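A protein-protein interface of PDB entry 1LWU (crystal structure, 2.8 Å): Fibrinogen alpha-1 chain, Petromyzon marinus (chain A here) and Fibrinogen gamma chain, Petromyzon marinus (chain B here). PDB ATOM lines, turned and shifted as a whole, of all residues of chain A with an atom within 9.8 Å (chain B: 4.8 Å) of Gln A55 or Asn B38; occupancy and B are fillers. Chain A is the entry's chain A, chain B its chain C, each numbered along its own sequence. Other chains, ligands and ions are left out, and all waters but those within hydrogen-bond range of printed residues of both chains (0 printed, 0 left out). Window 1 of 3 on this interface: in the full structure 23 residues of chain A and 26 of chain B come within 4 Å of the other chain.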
ATOM      1  N   LEU A  47      28.437 -17.872  27.996  1.00  0.00           N
ATOM      2  CA  LEU A  47      28.631 -19.300  28.199  1.00  0.00           C
ATOM      3  C   LEU A  47      27.276 -19.949  28.515  1.00  0.00           C
ATOM      4  O   LEU A  47      26.975 -21.039  28.041  1.00  0.00           O
ATOM      5  CB  LEU A  47      29.636 -19.512  29.350  1.00  0.00           C
ATOM      6  CG  LEU A  47      29.869 -20.865  30.049  1.00  0.00           C
ATOM      7  CD1 LEU A  47      28.674 -21.196  30.944  1.00  0.00           C
ATOM      8  CD2 LEU A  47      30.119 -21.975  29.025  1.00  0.00           C
ATOM      9  N   LEU A  48      26.458 -19.266  29.304  1.00  0.00           N
ATOM     10  CA  LEU A  48      25.144 -19.784  29.678  1.00  0.00           C
ATOM     11  C   LEU A  48      24.232 -19.803  28.455  1.00  0.00           C
ATOM     12  O   LEU A  48      23.199 -20.469  28.434  1.00  0.00           O
ATOM     13  CB  LEU A  48      24.534 -18.900  30.772  1.00  0.00           C
ATOM     14  CG  LEU A  48      23.318 -19.420  31.529  1.00  0.00           C
ATOM     15  CD1 LEU A  48      23.643 -20.758  32.162  1.00  0.00           C
ATOM     16  CD2 LEU A  48      22.928 -18.412  32.598  1.00  0.00           C
ATOM     17  N   GLN A  49      24.629 -19.057  27.435  1.00  0.00           N
ATOM     18  CA  GLN A  49      23.868 -18.969  26.199  1.00  0.00           C
ATOM     19  C   GLN A  49      24.190 -20.159  25.321  1.00  0.00           C
ATOM     20  O   GLN A  49      23.313 -20.749  24.694  1.00  0.00           O
ATOM     21  CB  GLN A  49      24.236 -17.688  25.466  1.00  0.00           C
ATOM     22  CG  GLN A  49      23.682 -17.578  24.066  1.00  0.00           C
ATOM     23  CD  GLN A  49      24.323 -16.442  23.307  1.00  0.00           C
ATOM     24  OE1 GLN A  49      25.528 -16.465  23.030  1.00  0.00           O
ATOM     25  NE2 GLN A  49      23.528 -15.431  22.977  1.00  0.00           N
ATOM     26  N   HIS A  50      25.468 -20.499  25.270  1.00  0.00           N
ATOM     27  CA  HIS A  50      25.899 -21.624  24.470  1.00  0.00           C
ATOM     28  C   HIS A  50      25.436 -22.943  25.079  1.00  0.00           C
ATOM     29  O   HIS A  50      25.316 -23.943  24.382  1.00  0.00           O
ATOM     30  CB  HIS A  50      27.414 -21.619  24.326  1.00  0.00           C
ATOM     31  CG  HIS A  50      27.919 -22.670  23.397  1.00  0.00           C
ATOM     32  ND1 HIS A  50      28.108 -23.978  23.787  1.00  0.00           N
ATOM     33  CD2 HIS A  50      28.205 -22.626  22.074  1.00  0.00           C
ATOM     34  CE1 HIS A  50      28.488 -24.695  22.745  1.00  0.00           C
ATOM     35  NE2 HIS A  50      28.554 -23.897  21.693  1.00  0.00           N
ATOM     36  N   ASN A  51      25.169 -22.948  26.379  1.00  0.00           N
ATOM     37  CA  ASN A  51      24.700 -24.157  27.028  1.00  0.00           C
ATOM     38  C   ASN A  51      23.202 -24.350  26.768  1.00  0.00           C
ATOM     39  O   ASN A  51      22.757 -25.458  26.444  1.00  0.00           O
ATOM     40  CB  ASN A  51      24.976 -24.103  28.533  1.00  0.00           C
ATOM     41  CG  ASN A  51      26.455 -24.241  28.869  1.00  0.00           C
ATOM     42  OD1 ASN A  51      26.829 -24.287  30.042  1.00  0.00           O
ATOM     43  ND2 ASN A  51      27.299 -24.302  27.845  1.00  0.00           N
ATOM     44  N   ILE A  52      22.420 -23.281  26.917  1.00  0.00           N
ATOM     45  CA  ILE A  52      20.994 -23.386  26.653  1.00  0.00           C
ATOM     46  C   ILE A  52      20.898 -23.819  25.199  1.00  0.00           C
ATOM     47  O   ILE A  52      20.059 -24.632  24.827  1.00  0.00           O
ATOM     48  CB  ILE A  52      20.279 -22.043  26.857  1.00  0.00           C
ATOM     49  CG1 ILE A  52      20.259 -21.704  28.349  1.00  0.00           C
ATOM     50  CG2 ILE A  52      18.853 -22.120  26.314  1.00  0.00           C
ATOM     51  CD1 ILE A  52      19.503 -20.429  28.692  1.00  0.00           C
ATOM     52  N   LYS A  53      21.790 -23.274  24.389  1.00  0.00           N
ATOM     53  CA  LYS A  53      21.866 -23.604  22.976  1.00  0.00           C
ATOM     54  C   LYS A  53      21.922 -25.109  22.804  1.00  0.00           C
ATOM     55  O   LYS A  53      21.127 -25.690  22.058  1.00  0.00           O
ATOM     56  CB  LYS A  53      23.131 -22.992  22.373  1.00  0.00           C
ATOM     57  CG  LYS A  53      23.569 -23.581  21.039  1.00  0.00           C
ATOM     58  CD  LYS A  53      22.713 -23.097  19.888  1.00  0.00           C
ATOM     59  CE  LYS A  53      23.334 -23.564  18.590  1.00  0.00           C
ATOM     60  NZ  LYS A  53      24.807 -23.314  18.592  1.00  0.00           N
ATOM     61  N   THR A  54      22.868 -25.733  23.502  1.00  0.00           N
ATOM     62  CA  THR A  54      23.053 -27.178  23.416  1.00  0.00           C
ATOM     63  C   THR A  54      22.304 -28.003  24.452  1.00  0.00           C
ATOM     64  O   THR A  54      22.789 -29.047  24.874  1.00  0.00           O
ATOM     65  CB  THR A  54      24.550 -27.563  23.487  1.00  0.00           C
ATOM     66  OG1 THR A  54      25.141 -26.982  24.654  1.00  0.00           O
ATOM     67  CG2 THR A  54      25.294 -27.078  22.247  1.00  0.00           C
ATOM     68  N   GLN A  55      21.133 -27.535  24.872  1.00  0.00           N
ATOM     69  CA  GLN A  55      20.309 -28.273  25.829  1.00  0.00           C
ATOM     70  C   GLN A  55      18.902 -28.276  25.261  1.00  0.00           C
ATOM     71  O   GLN A  55      18.107 -29.179  25.518  1.00  0.00           O
ATOM     72  CB  GLN A  55      20.295 -27.611  27.209  1.00  0.00           C
ATOM     73  CG  GLN A  55      19.620 -28.484  28.251  1.00  0.00           C
ATOM     74  CD  GLN A  55      19.475 -27.821  29.607  1.00  0.00           C
ATOM     75  OE1 GLN A  55      18.563 -27.023  29.827  1.00  0.00           O
ATOM     76  NE2 GLN A  55      20.375 -28.154  30.529  1.00  0.00           N
ATOM     77  N   VAL A  56      18.610 -27.239  24.485  1.00  0.00           N
ATOM     78  CA  VAL A  56      17.316 -27.090  23.837  1.00  0.00           C
ATOM     79  C   VAL A  56      17.330 -28.050  22.659  1.00  0.00           C
ATOM     80  O   VAL A  56      16.302 -28.599  22.264  1.00  0.00           O
ATOM     81  CB  VAL A  56      17.108 -25.642  23.311  1.00  0.00           C
ATOM     82  CG1 VAL A  56      15.787 -25.543  22.571  1.00  0.00           C
ATOM     83  CG2 VAL A  56      17.123 -24.661  24.460  1.00  0.00           C
ATOM     84  N   SER A  57      18.520 -28.239  22.101  1.00  0.00           N
ATOM     85  CA  SER A  57      18.703 -29.142  20.977  1.00  0.00           C
ATOM     86  C   SER A  57      18.608 -30.574  21.483  1.00  0.00           C
ATOM     87  O   SER A  57      17.855 -31.387  20.949  1.00  0.00           O
ATOM     88  CB  SER A  57      20.074 -28.909  20.337  1.00  0.00           C
ATOM     89  OG  SER A  57      20.448 -30.006  19.521  1.00  0.00           O
ATOM     90  N   GLN A  58      19.369 -30.863  22.533  1.00  0.00           N
ATOM     91  CA  GLN A  58      19.398 -32.189  23.125  1.00  0.00           C
ATOM     92  C   GLN A  58      18.026 -32.620  23.610  1.00  0.00           C
ATOM     93  O   GLN A  58      17.565 -33.716  23.283  1.00  0.00           O
ATOM     94  CB  GLN A  58      20.375 -32.223  24.293  1.00  0.00           C
ATOM     95  CG  GLN A  58      20.751 -33.617  24.725  1.00  0.00           C
ATOM     96  CD  GLN A  58      21.751 -33.610  25.859  1.00  0.00           C
ATOM     97  OE1 GLN A  58      22.638 -32.756  25.903  1.00  0.00           O
ATOM     98  NE2 GLN A  58      21.627 -34.567  26.777  1.00  0.00           N
ATOM     99  N   ILE A  59      17.373 -31.762  24.389  1.00  0.00           N
ATOM    100  CA  ILE A  59      16.058 -32.102  24.898  1.00  0.00           C
ATOM    101  C   ILE A  59      15.056 -32.283  23.780  1.00  0.00           C
ATOM    102  O   ILE A  59      14.149 -33.113  23.888  1.00  0.00           O
ATOM    103  CB  ILE A  59      15.531 -31.045  25.862  1.00  0.00           C
ATOM    104  CG1 ILE A  59      16.352 -31.086  27.145  1.00  0.00           C
ATOM    105  CG2 ILE A  59      14.064 -31.317  26.182  1.00  0.00           C
ATOM    106  CD1 ILE A  59      15.923 -30.096  28.177  1.00  0.00           C
ATOM    107  N   LEU A  60      15.206 -31.522  22.701  1.00  0.00           N
ATOM    108  CA  LEU A  60      14.270 -31.661  21.599  1.00  0.00           C
ATOM    109  C   LEU A  60      14.420 -33.035  20.985  1.00  0.00           C
ATOM    110  O   LEU A  60      13.443 -33.761  20.812  1.00  0.00           O
ATOM    111  CB  LEU A  60      14.509 -30.608  20.528  1.00  0.00           C
ATOM    112  CG  LEU A  60      13.657 -30.855  19.274  1.00  0.00           C
ATOM    113  CD1 LEU A  60      12.202 -31.210  19.684  1.00  0.00           C
ATOM    114  CD2 LEU A  60      13.733 -29.622  18.352  1.00  0.00           C
ATOM    115  N   ARG A  61      15.655 -33.382  20.646  1.00  0.00           N
ATOM    116  CA  ARG A  61      15.953 -34.678  20.058  1.00  0.00           C
ATOM    117  C   ARG A  61      15.352 -35.772  20.944  1.00  0.00           C
ATOM    118  O   ARG A  61      14.585 -36.622  20.477  1.00  0.00           O
ATOM    119  CB  ARG A  61      17.466 -34.868  19.956  1.00  0.00           C
ATOM    120  CG  ARG A  61      17.866 -36.243  19.487  1.00  0.00           C
ATOM    121  CD  ARG A  61      18.147 -36.296  17.991  1.00  0.00           C
ATOM    122  NE  ARG A  61      19.532 -35.933  17.707  1.00  0.00           N
ATOM    123  CZ  ARG A  61      20.003 -34.692  17.748  1.00  0.00           C
ATOM    124  NH1 ARG A  61      19.199 -33.683  18.052  1.00  0.00           N
ATOM    125  NH2 ARG A  61      21.285 -34.467  17.506  1.00  0.00           N
ATOM    126  N   VAL A  62      15.693 -35.729  22.229  1.00  0.00           N
ATOM    127  CA  VAL A  62      15.195 -36.714  23.176  1.00  0.00           C
ATOM    128  C   VAL A  62      13.682 -36.864  23.098  1.00  0.00           C
ATOM    129  O   VAL A  62      13.169 -37.972  23.037  1.00  0.00           O
ATOM    130  CB  VAL A  62      15.562 -36.343  24.618  1.00  0.00           C
ATOM    131  CG1 VAL A  62      15.160 -37.451  25.550  1.00  0.00           C
ATOM    132  CG2 VAL A  62      17.041 -36.095  24.726  1.00  0.00           C
ATOM    133  N   GLU A  63      12.963 -35.753  23.098  1.00  0.00           N
ATOM    134  CA  GLU A  63      11.518 -35.833  23.037  1.00  0.00           C
ATOM    135  C   GLU A  63      10.994 -36.575  21.823  1.00  0.00           C
ATOM    136  O   GLU A  63      10.012 -37.287  21.930  1.00  0.00           O
ATOM    137  CB  GLU A  63      10.888 -34.445  23.068  1.00  0.00           C
ATOM    138  CG  GLU A  63       9.371 -34.487  23.022  1.00  0.00           C
ATOM    139  CD  GLU A  63       8.780 -33.106  23.073  1.00  0.00           C
ATOM    140  OE1 GLU A  63       9.113 -32.296  22.181  1.00  0.00           O
ATOM    141  OE2 GLU A  63       7.990 -32.822  24.000  1.00  0.00           O
ATOM    142  N   ASN A  90       8.626 -22.878  22.041  1.00  0.00           N
ATOM    143  CA  ASN A  90       9.864 -22.954  22.788  1.00  0.00           C
ATOM    144  C   ASN A  90      11.031 -22.648  21.843  1.00  0.00           C
ATOM    145  O   ASN A  90      12.048 -22.116  22.267  1.00  0.00           O
ATOM    146  CB  ASN A  90      10.012 -24.354  23.396  1.00  0.00           C
ATOM    147  CG  ASN A  90      11.343 -24.553  24.095  1.00  0.00           C
ATOM    148  OD1 ASN A  90      12.392 -24.606  23.457  1.00  0.00           O
ATOM    149  ND2 ASN A  90      11.307 -24.659  25.417  1.00  0.00           N
ATOM    150  N   LEU A  91      10.879 -22.982  20.561  1.00  0.00           N
ATOM    151  CA  LEU A  91      11.938 -22.729  19.582  1.00  0.00           C
ATOM    152  C   LEU A  91      12.048 -21.243  19.259  1.00  0.00           C
ATOM    153  O   LEU A  91      13.087 -20.773  18.798  1.00  0.00           O
ATOM    154  CB  LEU A  91      11.701 -23.533  18.294  1.00  0.00           C
ATOM    155  CG  LEU A  91      11.851 -25.061  18.392  1.00  0.00           C
ATOM    156  CD1 LEU A  91      11.696 -25.688  17.005  1.00  0.00           C
ATOM    157  CD2 LEU A  91      13.217 -25.417  18.984  1.00  0.00           C
ATOM    158  N   GLU A  94      13.728 -19.883  22.498  1.00  0.00           N
ATOM    159  CA  GLU A  94      15.101 -20.367  22.467  1.00  0.00           C
ATOM    160  C   GLU A  94      15.920 -19.518  21.526  1.00  0.00           C
ATOM    161  O   GLU A  94      17.134 -19.374  21.706  1.00  0.00           O
ATOM    162  CB  GLU A  94      15.137 -21.827  22.001  1.00  0.00           C
ATOM    163  CG  GLU A  94      16.324 -22.197  21.095  1.00  0.00           C
ATOM    164  CD  GLU A  94      16.109 -21.822  19.626  1.00  0.00           C
ATOM    165  OE1 GLU A  94      15.173 -22.361  18.993  1.00  0.00           O
ATOM    166  OE2 GLU A  94      16.882 -20.991  19.104  1.00  0.00           O
ATOM    167  N   MET B  34      19.959 -24.268  37.710  1.00  0.00           N
ATOM    168  CA  MET B  34      18.804 -24.654  36.915  1.00  0.00           C
ATOM    169  C   MET B  34      19.215 -25.426  35.674  1.00  0.00           C
ATOM    170  O   MET B  34      18.526 -26.348  35.250  1.00  0.00           O
ATOM    171  CB  MET B  34      18.024 -23.405  36.512  1.00  0.00           C
ATOM    172  CG  MET B  34      16.532 -23.627  36.342  1.00  0.00           C
ATOM    173  SD  MET B  34      15.629 -22.067  36.222  1.00  0.00           S
ATOM    174  CE  MET B  34      16.081 -21.297  37.782  1.00  0.00           C
ATOM    175  N   TRP B  35      20.343 -25.053  35.091  1.00  0.00           N
ATOM    176  CA  TRP B  35      20.806 -25.735  33.899  1.00  0.00           C
ATOM    177  C   TRP B  35      21.376 -27.107  34.227  1.00  0.00           C
ATOM    178  O   TRP B  35      21.093 -28.086  33.528  1.00  0.00           O
ATOM    179  CB  TRP B  35      21.872 -24.911  33.188  1.00  0.00           C
ATOM    180  CG  TRP B  35      22.220 -25.479  31.852  1.00  0.00           C
ATOM    181  CD1 TRP B  35      21.478 -25.402  30.703  1.00  0.00           C
ATOM    182  CD2 TRP B  35      23.370 -26.268  31.534  1.00  0.00           C
ATOM    183  NE1 TRP B  35      22.096 -26.099  29.692  1.00  0.00           N
ATOM    184  CE2 TRP B  35      23.259 -26.640  30.175  1.00  0.00           C
ATOM    185  CE3 TRP B  35      24.483 -26.700  32.266  1.00  0.00           C
ATOM    186  CZ2 TRP B  35      24.221 -27.423  29.535  1.00  0.00           C
ATOM    187  CZ3 TRP B  35      25.435 -27.474  31.632  1.00  0.00           C
ATOM    188  CH2 TRP B  35      25.298 -27.829  30.278  1.00  0.00           C
ATOM    189  N   ARG B  36      22.190 -27.171  35.280  1.00  0.00           N
ATOM    190  CA  ARG B  36      22.800 -28.432  35.703  1.00  0.00           C
ATOM    191  C   ARG B  36      21.717 -29.448  36.071  1.00  0.00           C
ATOM    192  O   ARG B  36      21.795 -30.616  35.697  1.00  0.00           O
ATOM    193  CB  ARG B  36      23.742 -28.198  36.892  1.00  0.00           C
ATOM    194  CG  ARG B  36      25.122 -27.653  36.501  1.00  0.00           C
ATOM    195  CD  ARG B  36      25.840 -27.006  37.689  1.00  0.00           C
ATOM    196  NE  ARG B  36      25.335 -25.658  37.971  1.00  0.00           N
ATOM    197  CZ  ARG B  36      25.560 -24.985  39.099  1.00  0.00           C
ATOM    198  NH1 ARG B  36      26.284 -25.534  40.067  1.00  0.00           N
ATOM    199  NH2 ARG B  36      25.064 -23.764  39.255  1.00  0.00           N
ATOM    200  N   VAL B  37      20.709 -28.998  36.805  1.00  0.00           N
ATOM    201  CA  VAL B  37      19.610 -29.865  37.187  1.00  0.00           C
ATOM    202  C   VAL B  37      18.992 -30.444  35.922  1.00  0.00           C
ATOM    203  O   VAL B  37      18.824 -31.656  35.794  1.00  0.00           O
ATOM    204  CB  VAL B  37      18.544 -29.063  37.970  1.00  0.00           C
ATOM    205  CG1 VAL B  37      17.155 -29.722  37.847  1.00  0.00           C
ATOM    206  CG2 VAL B  37      18.972 -28.950  39.428  1.00  0.00           C
ATOM    207  N   ASN B  38      18.657 -29.563  34.987  1.00  0.00           N
ATOM    208  CA  ASN B  38      18.061 -29.972  33.725  1.00  0.00           C
ATOM    209  C   ASN B  38      18.956 -30.953  32.989  1.00  0.00           C
ATOM    210  O   ASN B  38      18.499 -32.020  32.572  1.00  0.00           O
ATOM    211  CB  ASN B  38      17.794 -28.742  32.849  1.00  0.00           C
ATOM    212  CG  ASN B  38      16.429 -28.139  33.100  1.00  0.00           C
ATOM    213  OD1 ASN B  38      15.897 -28.214  34.216  1.00  0.00           O
ATOM    214  ND2 ASN B  38      15.853 -27.528  32.066  1.00  0.00           N
ATOM    215  N   GLN B  39      20.230 -30.601  32.843  1.00  0.00           N
ATOM    216  CA  GLN B  39      21.163 -31.467  32.137  1.00  0.00           C
ATOM    217  C   GLN B  39      21.181 -32.867  32.751  1.00  0.00           C
ATOM    218  O   GLN B  39      21.552 -33.843  32.100  1.00  0.00           O
ATOM    219  CB  GLN B  39      22.563 -30.854  32.145  1.00  0.00           C
ATOM    220  CG  GLN B  39      23.426 -31.292  30.963  1.00  0.00           C
ATOM    221  CD  GLN B  39      22.750 -31.052  29.613  1.00  0.00           C
ATOM    222  OE1 GLN B  39      22.307 -29.941  29.315  1.00  0.00           O
ATOM    223  NE2 GLN B  39      22.675 -32.099  28.791  1.00  0.00           N
ATOM    224  N   GLN B  40      20.770 -32.962  34.009  1.00  0.00           N
ATOM    225  CA  GLN B  40      20.712 -34.242  34.686  1.00  0.00           C
ATOM    226  C   GLN B  40      19.394 -34.894  34.310  1.00  0.00           C
ATOM    227  O   GLN B  40      19.329 -36.102  34.087  1.00  0.00           O
ATOM    228  CB  GLN B  40      20.797 -34.041  36.190  1.00  0.00           C
ATOM    229  CG  GLN B  40      22.164 -33.535  36.641  1.00  0.00           C
ATOM    230  CD  GLN B  40      22.162 -33.015  38.078  1.00  0.00           C
ATOM    231  OE1 GLN B  40      23.209 -32.630  38.612  1.00  0.00           O
ATOM    232  NE2 GLN B  40      20.982 -32.995  38.708  1.00  0.00           N
ATOM    233  N   PHE B  41      18.345 -34.080  34.228  1.00  0.00           N
ATOM    234  CA  PHE B  41      17.010 -34.550  33.853  1.00  0.00           C
ATOM    235  C   PHE B  41      17.104 -35.211  32.472  1.00  0.00           C
ATOM    236  O   PHE B  41      16.514 -36.267  32.229  1.00  0.00           O
ATOM    237  CB  PHE B  41      16.042 -33.366  33.786  1.00  0.00           C
ATOM    238  CG  PHE B  41      14.597 -33.724  34.017  1.00  0.00           C
ATOM    239  CD1 PHE B  41      14.068 -34.920  33.561  1.00  0.00           C
ATOM    240  CD2 PHE B  41      13.745 -32.824  34.659  1.00  0.00           C
ATOM    241  CE1 PHE B  41      12.701 -35.220  33.737  1.00  0.00           C
ATOM    242  CE2 PHE B  41      12.374 -33.109  34.841  1.00  0.00           C
ATOM    243  CZ  PHE B  41      11.854 -34.308  34.378  1.00  0.00           C
ATOM    244  N   VAL B  42      17.845 -34.582  31.565  1.00  0.00           N
ATOM    245  CA  VAL B  42      18.019 -35.116  30.217  1.00  0.00           C
ATOM    246  C   VAL B  42      18.676 -36.491  30.284  1.00  0.00           C
ATOM    247  O   VAL B  42      18.342 -37.388  29.516  1.00  0.00           O
ATOM    248  CB  VAL B  42      18.896 -34.192  29.374  1.00  0.00           C
ATOM    249  CG1 VAL B  42      18.940 -34.682  27.945  1.00  0.00           C
ATOM    250  CG2 VAL B  42      18.354 -32.786  29.443  1.00  0.00           C
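The indole nitrogen of Trp B35 sits close to the side-chain amide nitrogen of Gln A55. The side-chain amide nitrogen (NE2) of Gln A55 sits at hydrogen-bond distance from the side-chain amide oxygen (OE1) of Gln B39 (2.9 Å). The indole nitrogen of Trp B35 sits at hydrogen-bond distance from the backbone carbonyl oxygen of Asn A51. NE2 of Gln B39 is in hydrogen-bond range of OE1 of Gln A58 (3.0 Å).
O of Asn A51 lies close to OG1 of Thr A54, 3.3 Å away. O of Leu A47 lies within hydrogen-bond range of ND2 of Asn A51 (3.3 Å). OD1 of Asn B38 lies close to O of Met B34, 3.4 Å away.
N of Ile A52 touches NE1 of Trp B35, 3.97 Å away. NE2 of Gln A55 touches CB of Asn B38 (3.5 Å). Val B42 touches Gln A58 (CG1 to NE2, 2.9 Å). CG2 of Val B42 touches CG1 of Ile A59, at 3.5 Å. Val A62 touches Val B42.
Printed residues of chain B within 4 Å of Ile A52: Trp B35 (3.97 Å). Gln A55 touches just these residues of chain B: Trp B35 (2.8 Å), Asn B38 (3.5 Å) and Gln B39 (2.9 Å). Of the printed residues of chain B, Ile A59 touches Val B42. Of the printed residues of chain B, Val A62 touches Val B42. Glu A63 touches none of the printed residues of chain B. Gln B39 touches just these residues of chain A: Gln A55 (2.9 Å) and Gln A58 (3.0 Å). The nearest residue of chain B that does not touch Gln A55 is Val B42 (4.6 Å).
Of the 20 printed residues of chain A, 6 touch a printed residue of chain B. Along chain A the printed residues that touch a printed residue of chain B span positions 51 to 62. Among the printed residues, 9 pairs touch across the chains. Among the printed residues, no Asp or Glu carboxylate lies within 4 Å of a Lys or Arg side-chain nitrogen of the other chain.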
